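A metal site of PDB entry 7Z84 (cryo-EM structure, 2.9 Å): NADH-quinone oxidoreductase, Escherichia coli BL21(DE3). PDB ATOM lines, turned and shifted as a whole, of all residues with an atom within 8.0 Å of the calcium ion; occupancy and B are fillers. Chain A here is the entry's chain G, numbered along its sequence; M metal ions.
The calcium ion is bound by OE1 of Gln 632 (2.5 Å). The calcium ion is bound by the side-chain carboxylate (OE2) of Glu 647. The calcium ion is bound by OD2 of Asp 731. The side-chain carboxylate (OD2) of Asp 617 is bound to the calcium ion, 2.9 Å away. The calcium ion has four donor atoms within binding distance.
Merely in contact with the calcium ion: Asp 729 (3.6 Å). Within 4 Å of the calcium ion: Asp 617, Gln 632, Glu 647, Asp 729 and Asp 731.
The backbone NH of Gln 632 is in hydrogen-bond range of the backbone carbonyl oxygen of Ser 616 (3.4 Å). NE of Arg 704 is in hydrogen-bond range of O of Gln 632 (2.7 Å). The side-chain amide nitrogen (NE2) of Gln 632 lies within hydrogen-bond range of the backbone carbonyl oxygen (O) of Tyr 634. The side-chain carboxylate of Glu 647 lies within salt-bridge range of the guanidinium group of Arg 650 (2.8 Å). The backbone NH of Asp 731 sits close to the side-chain carboxylate of Asp 729, at 3.5 Å. The side-chain carboxylate of Asp 731 lies within hydrogen-bond range of the backbone NH of Leu 669 (3.4 Å). The backbone carbonyl oxygen (O) of Asp 617 lies within hydrogen-bond range of the indole nitrogen (NE1) of Trp 649 (3.0 Å). The guanidinium group (NH2) of Arg 704 lies within salt-bridge range of the side-chain carboxylate (OD2) of Asp 729 (2.8 Å).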
ATOM      1  N   GLU A 615       7.189  12.000  20.639  1.00  0.00           N
ATOM      2  CA  GLU A 615       8.443  11.276  20.846  1.00  0.00           C
ATOM      3  C   GLU A 615       9.414  12.035  21.734  1.00  0.00           C
ATOM      4  O   GLU A 615      10.611  11.718  21.752  1.00  0.00           O
ATOM      5  CB  GLU A 615       9.090  10.960  19.498  1.00  0.00           C
ATOM      6  CG  GLU A 615       8.198  10.173  18.556  1.00  0.00           C
ATOM      7  CD  GLU A 615       7.804  10.953  17.325  1.00  0.00           C
ATOM      8  OE1 GLU A 615       8.203  12.132  17.215  1.00  0.00           O
ATOM      9  OE2 GLU A 615       7.102  10.390  16.463  1.00  0.00           O
ATOM     10  N   SER A 616       8.942  13.035  22.472  1.00  0.00           N
ATOM     11  CA  SER A 616       9.813  13.856  23.291  1.00  0.00           C
ATOM     12  C   SER A 616       9.103  14.254  24.576  1.00  0.00           C
ATOM     13  O   SER A 616       7.874  14.274  24.653  1.00  0.00           O
ATOM     14  CB  SER A 616      10.265  15.122  22.550  1.00  0.00           C
ATOM     15  OG  SER A 616       9.189  16.034  22.383  1.00  0.00           O
ATOM     16  N   ASP A 617       9.907  14.559  25.588  1.00  0.00           N
ATOM     17  CA  ASP A 617       9.453  15.184  26.812  1.00  0.00           C
ATOM     18  C   ASP A 617       9.865  16.651  26.803  1.00  0.00           C
ATOM     19  O   ASP A 617      10.792  17.044  26.077  1.00  0.00           O
ATOM     20  CB  ASP A 617      10.044  14.494  28.047  1.00  0.00           C
ATOM     21  CG  ASP A 617      10.094  12.983  27.906  1.00  0.00           C
ATOM     22  OD1 ASP A 617       9.063  12.327  28.163  1.00  0.00           O
ATOM     23  OD2 ASP A 617      11.154  12.462  27.511  1.00  0.00           O
ATOM     24  N   PHE A 631       5.007  14.505  28.205  1.00  0.00           N
ATOM     25  CA  PHE A 631       5.812  13.310  28.335  1.00  0.00           C
ATOM     26  C   PHE A 631       5.838  12.548  27.008  1.00  0.00           C
ATOM     27  O   PHE A 631       4.916  12.661  26.203  1.00  0.00           O
ATOM     28  CB  PHE A 631       5.269  12.395  29.448  1.00  0.00           C
ATOM     29  CG  PHE A 631       5.263  13.034  30.819  1.00  0.00           C
ATOM     30  CD1 PHE A 631       4.242  13.898  31.198  1.00  0.00           C
ATOM     31  CD2 PHE A 631       6.254  12.737  31.731  1.00  0.00           C
ATOM     32  CE1 PHE A 631       4.243  14.475  32.455  1.00  0.00           C
ATOM     33  CE2 PHE A 631       6.255  13.314  32.988  1.00  0.00           C
ATOM     34  CZ  PHE A 631       5.245  14.180  33.345  1.00  0.00           C
ATOM     35  N   GLN A 632       6.922  11.797  26.795  1.00  0.00           N
ATOM     36  CA  GLN A 632       7.067  11.029  25.568  1.00  0.00           C
ATOM     37  C   GLN A 632       6.079   9.875  25.537  1.00  0.00           C
ATOM     38  O   GLN A 632       5.854   9.196  26.547  1.00  0.00           O
ATOM     39  CB  GLN A 632       8.500  10.509  25.465  1.00  0.00           C
ATOM     40  CG  GLN A 632       8.771   9.602  24.284  1.00  0.00           C
ATOM     41  CD  GLN A 632      10.251   9.351  24.068  1.00  0.00           C
ATOM     42  OE1 GLN A 632      11.093   9.990  24.693  1.00  0.00           O
ATOM     43  NE2 GLN A 632      10.573   8.427  23.177  1.00  0.00           N
ATOM     44  N   VAL A 633       5.469   9.659  24.379  1.00  0.00           N
ATOM     45  CA  VAL A 633       4.457   8.609  24.231  1.00  0.00           C
ATOM     46  C   VAL A 633       5.095   7.268  23.913  1.00  0.00           C
ATOM     47  O   VAL A 633       4.727   6.244  24.504  1.00  0.00           O
ATOM     48  CB  VAL A 633       3.433   9.012  23.167  1.00  0.00           C
ATOM     49  CG1 VAL A 633       2.214   8.101  23.225  1.00  0.00           C
ATOM     50  CG2 VAL A 633       3.027  10.455  23.350  1.00  0.00           C
ATOM     51  N   TYR A 634       6.038   7.234  22.971  1.00  0.00           N
ATOM     52  CA  TYR A 634       6.606   5.970  22.522  1.00  0.00           C
ATOM     53  C   TYR A 634       8.051   6.183  22.113  1.00  0.00           C
ATOM     54  O   TYR A 634       8.489   7.303  21.822  1.00  0.00           O
ATOM     55  CB  TYR A 634       5.789   5.380  21.373  1.00  0.00           C
ATOM     56  CG  TYR A 634       5.891   6.139  20.063  1.00  0.00           C
ATOM     57  CD1 TYR A 634       5.157   7.303  19.857  1.00  0.00           C
ATOM     58  CD2 TYR A 634       6.693   5.684  19.026  1.00  0.00           C
ATOM     59  CE1 TYR A 634       5.244   8.000  18.669  1.00  0.00           C
ATOM     60  CE2 TYR A 634       6.783   6.368  17.835  1.00  0.00           C
ATOM     61  CZ  TYR A 634       6.060   7.517  17.661  1.00  0.00           C
ATOM     62  OH  TYR A 634       6.138   8.213  16.473  1.00  0.00           O
ATOM     63  N   ASP A 635       8.784   5.079  22.093  1.00  0.00           N
ATOM     64  CA  ASP A 635      10.150   5.082  21.578  1.00  0.00           C
ATOM     65  C   ASP A 635      10.116   4.913  20.067  1.00  0.00           C
ATOM     66  O   ASP A 635       9.601   3.905  19.580  1.00  0.00           O
ATOM     67  CB  ASP A 635      10.949   3.958  22.216  1.00  0.00           C
ATOM     68  CG  ASP A 635      12.439   4.057  21.942  1.00  0.00           C
ATOM     69  OD1 ASP A 635      12.910   5.138  21.530  1.00  0.00           O
ATOM     70  OD2 ASP A 635      13.154   3.053  22.152  1.00  0.00           O
ATOM     71  N   PRO A 636      10.622   5.892  19.291  1.00  0.00           N
ATOM     72  CA  PRO A 636      10.638   5.720  17.823  1.00  0.00           C
ATOM     73  C   PRO A 636      11.500   4.573  17.354  1.00  0.00           C
ATOM     74  O   PRO A 636      11.211   3.965  16.312  1.00  0.00           O
ATOM     75  CB  PRO A 636      11.166   7.067  17.312  1.00  0.00           C
ATOM     76  CG  PRO A 636      11.138   7.990  18.473  1.00  0.00           C
ATOM     77  CD  PRO A 636      11.159   7.183  19.723  1.00  0.00           C
ATOM     78  N   LEU A 646      15.909  11.865  18.288  1.00  0.00           N
ATOM     79  CA  LEU A 646      16.084  12.229  19.694  1.00  0.00           C
ATOM     80  C   LEU A 646      15.336  13.517  19.990  1.00  0.00           C
ATOM     81  O   LEU A 646      14.822  14.202  19.100  1.00  0.00           O
ATOM     82  CB  LEU A 646      17.568  12.384  20.027  1.00  0.00           C
ATOM     83  CG  LEU A 646      18.453  11.160  19.830  1.00  0.00           C
ATOM     84  CD1 LEU A 646      19.913  11.544  19.959  1.00  0.00           C
ATOM     85  CD2 LEU A 646      18.096  10.089  20.835  1.00  0.00           C
ATOM     86  N   GLU A 647      15.270  13.838  21.281  1.00  0.00           N
ATOM     87  CA  GLU A 647      14.731  15.111  21.718  1.00  0.00           C
ATOM     88  C   GLU A 647      15.632  16.250  21.244  1.00  0.00           C
ATOM     89  O   GLU A 647      16.841  16.082  21.071  1.00  0.00           O
ATOM     90  CB  GLU A 647      14.609  15.133  23.239  1.00  0.00           C
ATOM     91  CG  GLU A 647      13.530  14.219  23.797  1.00  0.00           C
ATOM     92  CD  GLU A 647      14.051  12.849  24.172  1.00  0.00           C
ATOM     93  OE1 GLU A 647      15.106  12.441  23.648  1.00  0.00           O
ATOM     94  OE2 GLU A 647      13.413  12.185  25.014  1.00  0.00           O
ATOM     95  N   TRP A 649      16.403  19.097  22.802  1.00  0.00           N
ATOM     96  CA  TRP A 649      17.351  19.506  23.814  1.00  0.00           C
ATOM     97  C   TRP A 649      18.468  18.487  23.963  1.00  0.00           C
ATOM     98  O   TRP A 649      19.607  18.864  24.256  1.00  0.00           O
ATOM     99  CB  TRP A 649      16.660  19.724  25.163  1.00  0.00           C
ATOM    100  CG  TRP A 649      15.630  18.711  25.506  1.00  0.00           C
ATOM    101  CD1 TRP A 649      14.297  18.773  25.250  1.00  0.00           C
ATOM    102  CD2 TRP A 649      15.855  17.485  26.208  1.00  0.00           C
ATOM    103  NE1 TRP A 649      13.669  17.647  25.733  1.00  0.00           N
ATOM    104  CE2 TRP A 649      14.606  16.834  26.329  1.00  0.00           C
ATOM    105  CE3 TRP A 649      16.985  16.855  26.746  1.00  0.00           C
ATOM    106  CZ2 TRP A 649      14.458  15.602  26.959  1.00  0.00           C
ATOM    107  CZ3 TRP A 649      16.836  15.635  27.358  1.00  0.00           C
ATOM    108  CH2 TRP A 649      15.591  15.021  27.461  1.00  0.00           C
ATOM    109  N   ARG A 650      18.165  17.200  23.745  1.00  0.00           N
ATOM    110  CA  ARG A 650      19.207  16.181  23.748  1.00  0.00           C
ATOM    111  C   ARG A 650      20.194  16.402  22.608  1.00  0.00           C
ATOM    112  O   ARG A 650      21.415  16.355  22.817  1.00  0.00           O
ATOM    113  CB  ARG A 650      18.572  14.792  23.628  1.00  0.00           C
ATOM    114  CG  ARG A 650      19.549  13.655  23.751  1.00  0.00           C
ATOM    115  CD  ARG A 650      18.880  12.410  24.279  1.00  0.00           C
ATOM    116  NE  ARG A 650      18.897  12.351  25.737  1.00  0.00           N
ATOM    117  CZ  ARG A 650      17.825  12.132  26.487  1.00  0.00           C
ATOM    118  NH1 ARG A 650      16.631  11.946  25.950  1.00  0.00           N
ATOM    119  NH2 ARG A 650      17.964  12.109  27.807  1.00  0.00           N
ATOM    120  N   LEU A 669      16.851  14.545  31.298  1.00  0.00           N
ATOM    121  CA  LEU A 669      15.907  15.665  31.177  1.00  0.00           C
ATOM    122  C   LEU A 669      15.930  16.573  32.399  1.00  0.00           C
ATOM    123  O   LEU A 669      15.852  17.805  32.273  1.00  0.00           O
ATOM    124  CB  LEU A 669      14.490  15.130  30.928  1.00  0.00           C
ATOM    125  CG  LEU A 669      13.334  16.125  31.082  1.00  0.00           C
ATOM    126  CD1 LEU A 669      13.343  17.170  29.984  1.00  0.00           C
ATOM    127  CD2 LEU A 669      11.998  15.406  31.125  1.00  0.00           C
ATOM    128  N   ARG A 704       2.541   3.453  31.184  1.00  0.00           N
ATOM    129  CA  ARG A 704       2.078   4.154  29.996  1.00  0.00           C
ATOM    130  C   ARG A 704       0.976   3.405  29.267  1.00  0.00           C
ATOM    131  O   ARG A 704       0.168   4.038  28.579  1.00  0.00           O
ATOM    132  CB  ARG A 704       3.240   4.382  29.027  1.00  0.00           C
ATOM    133  CG  ARG A 704       4.010   5.672  29.263  1.00  0.00           C
ATOM    134  CD  ARG A 704       4.930   5.985  28.100  1.00  0.00           C
ATOM    135  NE  ARG A 704       5.706   7.190  28.326  1.00  0.00           N
ATOM    136  CZ  ARG A 704       6.964   7.217  28.764  1.00  0.00           C
ATOM    137  NH1 ARG A 704       7.628   6.096  29.005  1.00  0.00           N
ATOM    138  NH2 ARG A 704       7.564   8.393  28.946  1.00  0.00           N
ATOM    139  N   GLN A 728      13.731   1.804  27.840  1.00  0.00           N
ATOM    140  CA  GLN A 728      13.916   2.421  29.136  1.00  0.00           C
ATOM    141  C   GLN A 728      13.714   3.927  29.041  1.00  0.00           C
ATOM    142  O   GLN A 728      14.130   4.559  28.060  1.00  0.00           O
ATOM    143  CB  GLN A 728      15.312   2.112  29.679  1.00  0.00           C
ATOM    144  CG  GLN A 728      15.565   0.629  29.905  1.00  0.00           C
ATOM    145  CD  GLN A 728      14.512  -0.004  30.797  1.00  0.00           C
ATOM    146  OE1 GLN A 728      13.816  -0.933  30.380  1.00  0.00           O
ATOM    147  NE2 GLN A 728      14.408   0.484  32.029  1.00  0.00           N
ATOM    148  N   ASP A 729      13.076   4.497  30.052  1.00  0.00           N
ATOM    149  CA  ASP A 729      12.790   5.925  30.112  1.00  0.00           C
ATOM    150  C   ASP A 729      13.588   6.508  31.273  1.00  0.00           C
ATOM    151  O   ASP A 729      13.132   6.493  32.425  1.00  0.00           O
ATOM    152  CB  ASP A 729      11.300   6.187  30.264  1.00  0.00           C
ATOM    153  CG  ASP A 729      10.948   7.649  30.069  1.00  0.00           C
ATOM    154  OD1 ASP A 729      11.764   8.391  29.485  1.00  0.00           O
ATOM    155  OD2 ASP A 729       9.846   8.059  30.505  1.00  0.00           O
ATOM    156  N   ILE A 730      14.779   7.019  30.978  1.00  0.00           N
ATOM    157  CA  ILE A 730      15.604   7.656  32.001  1.00  0.00           C
ATOM    158  C   ILE A 730      15.225   9.106  32.231  1.00  0.00           C
ATOM    159  O   ILE A 730      15.721   9.721  33.184  1.00  0.00           O
ATOM    160  CB  ILE A 730      17.101   7.571  31.643  1.00  0.00           C
ATOM    161  CG1 ILE A 730      17.390   8.356  30.369  1.00  0.00           C
ATOM    162  CG2 ILE A 730      17.528   6.119  31.478  1.00  0.00           C
ATOM    163  CD1 ILE A 730      18.810   8.848  30.265  1.00  0.00           C
ATOM    164  N   ASP A 731      14.366   9.665  31.381  1.00  0.00           N
ATOM    165  CA  ASP A 731      14.040  11.090  31.448  1.00  0.00           C
ATOM    166  C   ASP A 731      12.922  11.395  32.428  1.00  0.00           C
ATOM    167  O   ASP A 731      12.977  12.421  33.125  1.00  0.00           O
ATOM    168  CB  ASP A 731      13.652  11.598  30.053  1.00  0.00           C
ATOM    169  CG  ASP A 731      14.831  11.620  29.103  1.00  0.00           C
ATOM    170  OD1 ASP A 731      15.984  11.706  29.574  1.00  0.00           O
ATOM    171  OD2 ASP A 731      14.601  11.562  27.871  1.00  0.00           O
ATOM    172  N   THR A 732      11.906  10.543  32.494  1.00  0.00           N
ATOM    173  CA  THR A 732      10.697  10.837  33.273  1.00  0.00           C
ATOM    174  C   THR A 732      10.379   9.642  34.167  1.00  0.00           C
ATOM    175  O   THR A 732      11.058   8.609  34.147  1.00  0.00           O
ATOM    176  CB  THR A 732       9.516  11.171  32.360  1.00  0.00           C
ATOM    177  OG1 THR A 732       9.382  10.156  31.350  1.00  0.00           O
ATOM    178  CG2 THR A 732       9.738  12.507  31.686  1.00  0.00           C
ATOM    179  N   PHE A 736       7.873   2.544  29.707  1.00  0.00           N
ATOM    180  CA  PHE A 736       7.306   2.114  28.441  1.00  0.00           C
ATOM    181  C   PHE A 736       6.769   0.696  28.533  1.00  0.00           C
ATOM    182  O   PHE A 736       7.127  -0.168  27.718  1.00  0.00           O
ATOM    183  CB  PHE A 736       8.360   2.189  27.331  1.00  0.00           C
ATOM    184  CG  PHE A 736       8.710   3.594  26.912  1.00  0.00           C
ATOM    185  CD1 PHE A 736       7.833   4.344  26.142  1.00  0.00           C
ATOM    186  CD2 PHE A 736       9.912   4.163  27.284  1.00  0.00           C
ATOM    187  CE1 PHE A 736       8.155   5.621  25.752  1.00  0.00           C
ATOM    188  CE2 PHE A 736      10.244   5.442  26.895  1.00  0.00           C
ATOM    189  CZ  PHE A 736       9.360   6.173  26.133  1.00  0.00           C
HETATM  190 CA    CA M   1      12.767  10.281  26.578  1.00  0.00          CA
